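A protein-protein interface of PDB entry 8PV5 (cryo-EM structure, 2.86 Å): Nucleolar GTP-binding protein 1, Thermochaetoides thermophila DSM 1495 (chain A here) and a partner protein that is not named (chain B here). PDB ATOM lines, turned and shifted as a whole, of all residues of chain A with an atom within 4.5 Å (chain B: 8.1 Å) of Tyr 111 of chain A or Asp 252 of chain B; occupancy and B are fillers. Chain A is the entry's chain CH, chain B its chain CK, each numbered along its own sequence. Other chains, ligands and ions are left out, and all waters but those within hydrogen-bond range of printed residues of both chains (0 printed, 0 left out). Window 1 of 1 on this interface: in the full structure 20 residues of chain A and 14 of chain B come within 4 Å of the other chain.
O of Asp 252 of chain B sits at hydrogen-bond distance from OH of Tyr 111 of chain A.
Asp 110 of chain A touches none of the printed residues of chain B.
Printed residues of chain B within 4 Å of Arg 113 of chain A: Gly 176 (3.8 Å).
Printed residues of chain B within 4 Å of Leu 114 of chain A: Gly 176, Tyr 179 and Gly 253.
Of the printed residues of chain B, Leu 127 of chain A touches Glu 250 (3.9 Å) and Asn 251 (3.6 Å).
Of the printed residues of chain A, Tyr 179 of chain B touches Leu 114 (3.6 Å).
Of the printed residues of chain A, Asp 252 of chain B touches Tyr 111 (2.6 Å) and Ala 130 (3.6 Å).
Asn 256 of chain B touches none of the printed residues of chain A.
The nearest residue of chain B that does not touch Tyr 111 of chain A is Cys 254 of chain B (4.9 Å).
The nearest printed residue of chain A that does not touch Asp 252 of chain B is Leu 127 of chain A (4.5 Å).
Among the printed residues, pairs that only touch across the chains: Leu 114 of chain A with Gly 176 of chain B, Leu 127 of chain A with Asn 251 of chain B, Ala 130 of chain A with Asp 252 of chain B, Leu 114 of chain A with Tyr 179 of chain B, Leu 114 of chain A with Gly 253 of chain B, Arg 113 of chain A with Gly 176 of chain B, Tyr 111 of chain A with Gly 253 of chain B and Leu 127 of chain A with Glu 250 of chain B.
OD1 of Asp 110 of chain A lies within salt-bridge range of NH1 of Arg 113 of chain A.
OH of Tyr 179 of chain B sits at hydrogen-bond distance from O of Gly 253 of chain B (3.0 Å).
OD1 of Asp 252 of chain B is in hydrogen-bond range of ND2 of Asn 247 of chain B.
The side-chain carboxylate of Glu 250 of chain B sits close to the side-chain amide oxygen of Asn 248 of chain B, 3.4 Å away.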
ATOM      1  N   ILE A 107      15.236  35.561  -5.528  1.00  0.00           N
ATOM      2  CA  ILE A 107      14.397  34.426  -5.904  1.00  0.00           C
ATOM      3  C   ILE A 107      12.923  34.789  -5.769  1.00  0.00           C
ATOM      4  O   ILE A 107      12.093  34.434  -6.619  1.00  0.00           O
ATOM      5  CB  ILE A 107      14.769  33.191  -5.059  1.00  0.00           C
ATOM      6  CG1 ILE A 107      16.069  32.578  -5.578  1.00  0.00           C
ATOM      7  CG2 ILE A 107      13.660  32.147  -5.051  1.00  0.00           C
ATOM      8  CD1 ILE A 107      16.574  31.433  -4.746  1.00  0.00           C
ATOM      9  N   SER A 108      12.583  35.538  -4.715  1.00  0.00           N
ATOM     10  CA  SER A 108      11.208  35.985  -4.527  1.00  0.00           C
ATOM     11  C   SER A 108      10.759  36.907  -5.654  1.00  0.00           C
ATOM     12  O   SER A 108       9.637  36.782  -6.155  1.00  0.00           O
ATOM     13  CB  SER A 108      11.070  36.687  -3.184  1.00  0.00           C
ATOM     14  OG  SER A 108       9.739  37.124  -2.971  1.00  0.00           O
ATOM     15  N   ARG A 109      11.624  37.842  -6.063  1.00  0.00           N
ATOM     16  CA  ARG A 109      11.270  38.742  -7.162  1.00  0.00           C
ATOM     17  C   ARG A 109      11.068  37.979  -8.466  1.00  0.00           C
ATOM     18  O   ARG A 109      10.103  38.237  -9.203  1.00  0.00           O
ATOM     19  CB  ARG A 109      12.343  39.816  -7.335  1.00  0.00           C
ATOM     20  CG  ARG A 109      12.403  40.828  -6.208  1.00  0.00           C
ATOM     21  CD  ARG A 109      13.172  42.068  -6.629  1.00  0.00           C
ATOM     22  NE  ARG A 109      14.480  41.743  -7.185  1.00  0.00           N
ATOM     23  CZ  ARG A 109      15.614  41.777  -6.501  1.00  0.00           C
ATOM     24  NH1 ARG A 109      15.641  42.121  -5.223  1.00  0.00           N
ATOM     25  NH2 ARG A 109      16.751  41.461  -7.112  1.00  0.00           N
ATOM     26  N   ASP A 110      11.953  37.018  -8.754  1.00  0.00           N
ATOM     27  CA  ASP A 110      11.828  36.224  -9.976  1.00  0.00           C
ATOM     28  C   ASP A 110      10.540  35.408  -9.979  1.00  0.00           C
ATOM     29  O   ASP A 110       9.835  35.337 -10.996  1.00  0.00           O
ATOM     30  CB  ASP A 110      13.041  35.310 -10.134  1.00  0.00           C
ATOM     31  CG  ASP A 110      14.303  36.070 -10.481  1.00  0.00           C
ATOM     32  OD1 ASP A 110      14.196  37.239 -10.906  1.00  0.00           O
ATOM     33  OD2 ASP A 110      15.404  35.499 -10.332  1.00  0.00           O
ATOM     34  N   TYR A 111      10.198  34.800  -8.843  1.00  0.00           N
ATOM     35  CA  TYR A 111       9.000  33.970  -8.823  1.00  0.00           C
ATOM     36  C   TYR A 111       7.717  34.791  -8.780  1.00  0.00           C
ATOM     37  O   TYR A 111       6.688  34.327  -9.275  1.00  0.00           O
ATOM     38  CB  TYR A 111       9.067  32.977  -7.666  1.00  0.00           C
ATOM     39  CG  TYR A 111       9.819  31.728  -8.055  1.00  0.00           C
ATOM     40  CD1 TYR A 111       9.174  30.682  -8.697  1.00  0.00           C
ATOM     41  CD2 TYR A 111      11.179  31.607  -7.811  1.00  0.00           C
ATOM     42  CE1 TYR A 111       9.857  29.547  -9.072  1.00  0.00           C
ATOM     43  CE2 TYR A 111      11.872  30.472  -8.178  1.00  0.00           C
ATOM     44  CZ  TYR A 111      11.205  29.445  -8.807  1.00  0.00           C
ATOM     45  OH  TYR A 111      11.887  28.310  -9.177  1.00  0.00           O
ATOM     46  N   VAL A 112       7.754  36.010  -8.235  1.00  0.00           N
ATOM     47  CA  VAL A 112       6.613  36.915  -8.374  1.00  0.00           C
ATOM     48  C   VAL A 112       6.415  37.302  -9.839  1.00  0.00           C
ATOM     49  O   VAL A 112       5.282  37.335 -10.344  1.00  0.00           O
ATOM     50  CB  VAL A 112       6.796  38.146  -7.465  1.00  0.00           C
ATOM     51  CG1 VAL A 112       5.833  39.257  -7.840  1.00  0.00           C
ATOM     52  CG2 VAL A 112       6.567  37.759  -6.016  1.00  0.00           C
ATOM     53  N   ARG A 113       7.517  37.566 -10.549  1.00  0.00           N
ATOM     54  CA  ARG A 113       7.429  37.880 -11.973  1.00  0.00           C
ATOM     55  C   ARG A 113       6.868  36.710 -12.775  1.00  0.00           C
ATOM     56  O   ARG A 113       6.112  36.911 -13.733  1.00  0.00           O
ATOM     57  CB  ARG A 113       8.804  38.278 -12.499  1.00  0.00           C
ATOM     58  CG  ARG A 113       8.787  38.988 -13.835  1.00  0.00           C
ATOM     59  CD  ARG A 113      10.171  39.490 -14.196  1.00  0.00           C
ATOM     60  NE  ARG A 113      10.747  40.320 -13.144  1.00  0.00           N
ATOM     61  CZ  ARG A 113      11.808  39.988 -12.422  1.00  0.00           C
ATOM     62  NH1 ARG A 113      12.443  38.844 -12.613  1.00  0.00           N
ATOM     63  NH2 ARG A 113      12.239  40.822 -11.480  1.00  0.00           N
ATOM     64  N   LEU A 114       7.231  35.480 -12.404  1.00  0.00           N
ATOM     65  CA  LEU A 114       6.671  34.314 -13.089  1.00  0.00           C
ATOM     66  C   LEU A 114       5.206  34.095 -12.718  1.00  0.00           C
ATOM     67  O   LEU A 114       4.403  33.644 -13.549  1.00  0.00           O
ATOM     68  CB  LEU A 114       7.494  33.069 -12.772  1.00  0.00           C
ATOM     69  CG  LEU A 114       8.942  33.083 -13.258  1.00  0.00           C
ATOM     70  CD1 LEU A 114       9.637  31.800 -12.864  1.00  0.00           C
ATOM     71  CD2 LEU A 114       9.008  33.298 -14.758  1.00  0.00           C
ATOM     72  N   LEU A 115       4.840  34.398 -11.470  1.00  0.00           N
ATOM     73  CA  LEU A 115       3.454  34.252 -11.042  1.00  0.00           C
ATOM     74  C   LEU A 115       2.549  35.272 -11.713  1.00  0.00           C
ATOM     75  O   LEU A 115       1.334  35.058 -11.797  1.00  0.00           O
ATOM     76  CB  LEU A 115       3.361  34.377  -9.522  1.00  0.00           C
ATOM     77  CG  LEU A 115       3.640  33.102  -8.730  1.00  0.00           C
ATOM     78  CD1 LEU A 115       3.749  33.405  -7.251  1.00  0.00           C
ATOM     79  CD2 LEU A 115       2.551  32.088  -8.983  1.00  0.00           C
ATOM     80  N   LEU A 127       5.089  26.927  -8.886  1.00  0.00           N
ATOM     81  CA  LEU A 127       5.997  28.063  -8.739  1.00  0.00           C
ATOM     82  C   LEU A 127       6.185  28.452  -7.274  1.00  0.00           C
ATOM     83  O   LEU A 127       7.307  28.765  -6.850  1.00  0.00           O
ATOM     84  CB  LEU A 127       5.487  29.252  -9.548  1.00  0.00           C
ATOM     85  CG  LEU A 127       5.630  29.159 -11.067  1.00  0.00           C
ATOM     86  CD1 LEU A 127       4.826  30.252 -11.744  1.00  0.00           C
ATOM     87  CD2 LEU A 127       7.089  29.234 -11.475  1.00  0.00           C
ATOM     88  N   ALA A 130       8.327  25.876  -5.661  1.00  0.00           N
ATOM     89  CA  ALA A 130       9.697  26.036  -6.133  1.00  0.00           C
ATOM     90  C   ALA A 130      10.406  27.169  -5.405  1.00  0.00           C
ATOM     91  O   ALA A 130      11.560  27.021  -4.979  1.00  0.00           O
ATOM     92  CB  ALA A 130       9.701  26.271  -7.642  1.00  0.00           C
ATOM     93  N   ALA A 131       9.724  28.305  -5.236  1.00  0.00           N
ATOM     94  CA  ALA A 131      10.314  29.433  -4.521  1.00  0.00           C
ATOM     95  C   ALA A 131      10.590  29.082  -3.063  1.00  0.00           C
ATOM     96  O   ALA A 131      11.669  29.383  -2.531  1.00  0.00           O
ATOM     97  CB  ALA A 131       9.396  30.650  -4.617  1.00  0.00           C
ATOM     98  N   ARG A 134      13.564  26.663  -2.844  1.00  0.00           N
ATOM     99  CA  ARG A 134      14.844  27.328  -3.073  1.00  0.00           C
ATOM    100  C   ARG A 134      15.265  28.164  -1.870  1.00  0.00           C
ATOM    101  O   ARG A 134      16.445  28.157  -1.490  1.00  0.00           O
ATOM    102  CB  ARG A 134      14.773  28.173  -4.342  1.00  0.00           C
ATOM    103  CG  ARG A 134      14.719  27.323  -5.593  1.00  0.00           C
ATOM    104  CD  ARG A 134      14.714  28.135  -6.865  1.00  0.00           C
ATOM    105  NE  ARG A 134      15.914  28.946  -7.008  1.00  0.00           N
ATOM    106  CZ  ARG A 134      16.273  29.553  -8.130  1.00  0.00           C
ATOM    107  NH1 ARG A 134      15.588  29.393  -9.250  1.00  0.00           N
ATOM    108  NH2 ARG A 134      17.344  30.339  -8.129  1.00  0.00           N
ATOM    109  N   PRO B 154       8.018  29.620 -21.191  1.00  0.00           N
ATOM    110  CA  PRO B 154       9.296  30.325 -21.368  1.00  0.00           C
ATOM    111  C   PRO B 154       9.846  30.203 -22.782  1.00  0.00           C
ATOM    112  O   PRO B 154       9.722  29.165 -23.434  1.00  0.00           O
ATOM    113  CB  PRO B 154      10.215  29.645 -20.349  1.00  0.00           C
ATOM    114  CG  PRO B 154       9.299  29.156 -19.304  1.00  0.00           C
ATOM    115  CD  PRO B 154       8.069  28.714 -20.028  1.00  0.00           C
ATOM    116  N   GLY B 176       9.678  38.734 -18.854  1.00  0.00           N
ATOM    117  CA  GLY B 176       9.779  37.973 -17.624  1.00  0.00           C
ATOM    118  C   GLY B 176       9.826  36.475 -17.817  1.00  0.00           C
ATOM    119  O   GLY B 176      10.043  35.751 -16.839  1.00  0.00           O
ATOM    120  N   TYR B 179      14.567  33.226 -21.081  1.00  0.00           N
ATOM    121  CA  TYR B 179      15.672  32.573 -20.399  1.00  0.00           C
ATOM    122  C   TYR B 179      16.906  32.560 -21.291  1.00  0.00           C
ATOM    123  O   TYR B 179      16.807  32.425 -22.513  1.00  0.00           O
ATOM    124  CB  TYR B 179      15.310  31.140 -19.998  1.00  0.00           C
ATOM    125  CG  TYR B 179      14.451  31.050 -18.759  1.00  0.00           C
ATOM    126  CD1 TYR B 179      13.078  31.238 -18.827  1.00  0.00           C
ATOM    127  CD2 TYR B 179      15.015  30.780 -17.520  1.00  0.00           C
ATOM    128  CE1 TYR B 179      12.290  31.155 -17.696  1.00  0.00           C
ATOM    129  CE2 TYR B 179      14.235  30.698 -16.384  1.00  0.00           C
ATOM    130  CZ  TYR B 179      12.875  30.886 -16.478  1.00  0.00           C
ATOM    131  OH  TYR B 179      12.096  30.804 -15.349  1.00  0.00           O
ATOM    132  N   ILE B 245      15.872  19.319 -22.976  1.00  0.00           N
ATOM    133  CA  ILE B 245      15.293  19.831 -21.741  1.00  0.00           C
ATOM    134  C   ILE B 245      14.491  18.725 -21.069  1.00  0.00           C
ATOM    135  O   ILE B 245      13.603  18.118 -21.681  1.00  0.00           O
ATOM    136  CB  ILE B 245      14.428  21.066 -22.023  1.00  0.00           C
ATOM    137  CG1 ILE B 245      15.291  22.194 -22.590  1.00  0.00           C
ATOM    138  CG2 ILE B 245      13.723  21.522 -20.758  1.00  0.00           C
ATOM    139  CD1 ILE B 245      14.512  23.427 -22.974  1.00  0.00           C
ATOM    140  N   THR B 246      14.803  18.458 -19.802  1.00  0.00           N
ATOM    141  CA  THR B 246      14.239  17.331 -19.075  1.00  0.00           C
ATOM    142  C   THR B 246      13.253  17.734 -17.989  1.00  0.00           C
ATOM    143  O   THR B 246      12.809  16.868 -17.229  1.00  0.00           O
ATOM    144  CB  THR B 246      15.364  16.494 -18.458  1.00  0.00           C
ATOM    145  OG1 THR B 246      16.191  17.332 -17.644  1.00  0.00           O
ATOM    146  CG2 THR B 246      16.210  15.872 -19.550  1.00  0.00           C
ATOM    147  N   ASN B 247      12.897  19.011 -17.895  1.00  0.00           N
ATOM    148  CA  ASN B 247      11.956  19.487 -16.892  1.00  0.00           C
ATOM    149  C   ASN B 247      10.895  20.347 -17.564  1.00  0.00           C
ATOM    150  O   ASN B 247      10.878  20.516 -18.785  1.00  0.00           O
ATOM    151  CB  ASN B 247      12.668  20.278 -15.790  1.00  0.00           C
ATOM    152  CG  ASN B 247      13.159  21.629 -16.264  1.00  0.00           C
ATOM    153  OD1 ASN B 247      13.717  21.753 -17.353  1.00  0.00           O
ATOM    154  ND2 ASN B 247      12.950  22.655 -15.449  1.00  0.00           N
ATOM    155  N   ASN B 248      10.002  20.902 -16.746  1.00  0.00           N
ATOM    156  CA  ASN B 248       9.006  21.858 -17.213  1.00  0.00           C
ATOM    157  C   ASN B 248       9.379  23.237 -16.689  1.00  0.00           C
ATOM    158  O   ASN B 248       9.149  23.532 -15.506  1.00  0.00           O
ATOM    159  CB  ASN B 248       7.605  21.462 -16.742  1.00  0.00           C
ATOM    160  CG  ASN B 248       7.094  20.209 -17.421  1.00  0.00           C
ATOM    161  OD1 ASN B 248       7.016  20.142 -18.646  1.00  0.00           O
ATOM    162  ND2 ASN B 248       6.741  19.208 -16.627  1.00  0.00           N
ATOM    163  N   PRO B 249       9.985  24.098 -17.513  1.00  0.00           N
ATOM    164  CA  PRO B 249      10.390  25.428 -17.029  1.00  0.00           C
ATOM    165  C   PRO B 249       9.230  26.305 -16.594  1.00  0.00           C
ATOM    166  O   PRO B 249       9.403  27.130 -15.688  1.00  0.00           O
ATOM    167  CB  PRO B 249      11.129  26.025 -18.235  1.00  0.00           C
ATOM    168  CG  PRO B 249      11.557  24.845 -19.042  1.00  0.00           C
ATOM    169  CD  PRO B 249      10.454  23.848 -18.885  1.00  0.00           C
ATOM    170  N   GLU B 250       8.053  26.140 -17.203  1.00  0.00           N
ATOM    171  CA  GLU B 250       6.899  26.956 -16.838  1.00  0.00           C
ATOM    172  C   GLU B 250       6.412  26.647 -15.428  1.00  0.00           C
ATOM    173  O   GLU B 250       5.868  27.528 -14.754  1.00  0.00           O
ATOM    174  CB  GLU B 250       5.771  26.758 -17.855  1.00  0.00           C
ATOM    175  CG  GLU B 250       5.189  25.349 -17.923  1.00  0.00           C
ATOM    176  CD  GLU B 250       5.964  24.431 -18.850  1.00  0.00           C
ATOM    177  OE1 GLU B 250       6.957  24.890 -19.449  1.00  0.00           O
ATOM    178  OE2 GLU B 250       5.575  23.253 -18.984  1.00  0.00           O
ATOM    179  N   ASN B 251       6.605  25.414 -14.961  1.00  0.00           N
ATOM    180  CA  ASN B 251       6.230  25.035 -13.608  1.00  0.00           C
ATOM    181  C   ASN B 251       7.369  25.169 -12.611  1.00  0.00           C
ATOM    182  O   ASN B 251       7.108  25.391 -11.425  1.00  0.00           O
ATOM    183  CB  ASN B 251       5.720  23.589 -13.579  1.00  0.00           C
ATOM    184  CG  ASN B 251       4.367  23.433 -14.237  1.00  0.00           C
ATOM    185  OD1 ASN B 251       3.688  24.414 -14.532  1.00  0.00           O
ATOM    186  ND2 ASN B 251       3.966  22.190 -14.470  1.00  0.00           N
ATOM    187  N   ASP B 252       8.618  25.052 -13.058  1.00  0.00           N
ATOM    188  CA  ASP B 252       9.745  24.994 -12.139  1.00  0.00           C
ATOM    189  C   ASP B 252      10.486  26.314 -11.985  1.00  0.00           C
ATOM    190  O   ASP B 252      11.128  26.522 -10.949  1.00  0.00           O
ATOM    191  CB  ASP B 252      10.734  23.915 -12.591  1.00  0.00           C
ATOM    192  CG  ASP B 252      10.100  22.543 -12.655  1.00  0.00           C
ATOM    193  OD1 ASP B 252      10.639  21.668 -13.365  1.00  0.00           O
ATOM    194  OD2 ASP B 252       9.060  22.337 -11.995  1.00  0.00           O
ATOM    195  N   GLY B 253      10.419  27.208 -12.967  1.00  0.00           N
ATOM    196  CA  GLY B 253      11.171  28.438 -12.887  1.00  0.00           C
ATOM    197  C   GLY B 253      12.624  28.324 -13.276  1.00  0.00           C
ATOM    198  O   GLY B 253      13.379  29.284 -13.085  1.00  0.00           O
ATOM    199  N   CYS B 254      13.044  27.181 -13.812  1.00  0.00           N
ATOM    200  CA  CYS B 254      14.413  26.997 -14.265  1.00  0.00           C
ATOM    201  C   CYS B 254      14.413  25.992 -15.404  1.00  0.00           C
ATOM    202  O   CYS B 254      13.503  25.168 -15.532  1.00  0.00           O
ATOM    203  CB  CYS B 254      15.328  26.521 -13.131  1.00  0.00           C
ATOM    204  SG  CYS B 254      14.872  24.918 -12.429  1.00  0.00           S
ATOM    205  N   VAL B 255      15.450  26.062 -16.232  1.00  0.00           N
ATOM    206  CA  VAL B 255      15.615  25.161 -17.365  1.00  0.00           C
ATOM    207  C   VAL B 255      16.697  24.155 -17.006  1.00  0.00           C
ATOM    208  O   VAL B 255      17.840  24.533 -16.723  1.00  0.00           O
ATOM    209  CB  VAL B 255      15.974  25.921 -18.651  1.00  0.00           C
ATOM    210  CG1 VAL B 255      15.989  24.972 -19.835  1.00  0.00           C
ATOM    211  CG2 VAL B 255      14.998  27.059 -18.886  1.00  0.00           C
ATOM    212  N   ASN B 256      16.333  22.877 -17.004  1.00  0.00           N
ATOM    213  CA  ASN B 256      17.262  21.786 -16.758  1.00  0.00           C
ATOM    214  C   ASN B 256      17.393  20.947 -18.019  1.00  0.00           C
ATOM    215  O   ASN B 256      16.390  20.560 -18.623  1.00  0.00           O
ATOM    216  CB  ASN B 256      16.792  20.908 -15.597  1.00  0.00           C
ATOM    217  CG  ASN B 256      16.676  21.673 -14.300  1.00  0.00           C
ATOM    218  OD1 ASN B 256      17.301  22.718 -14.124  1.00  0.00           O
ATOM    219  ND2 ASN B 256      15.873  21.157 -13.380  1.00  0.00           N
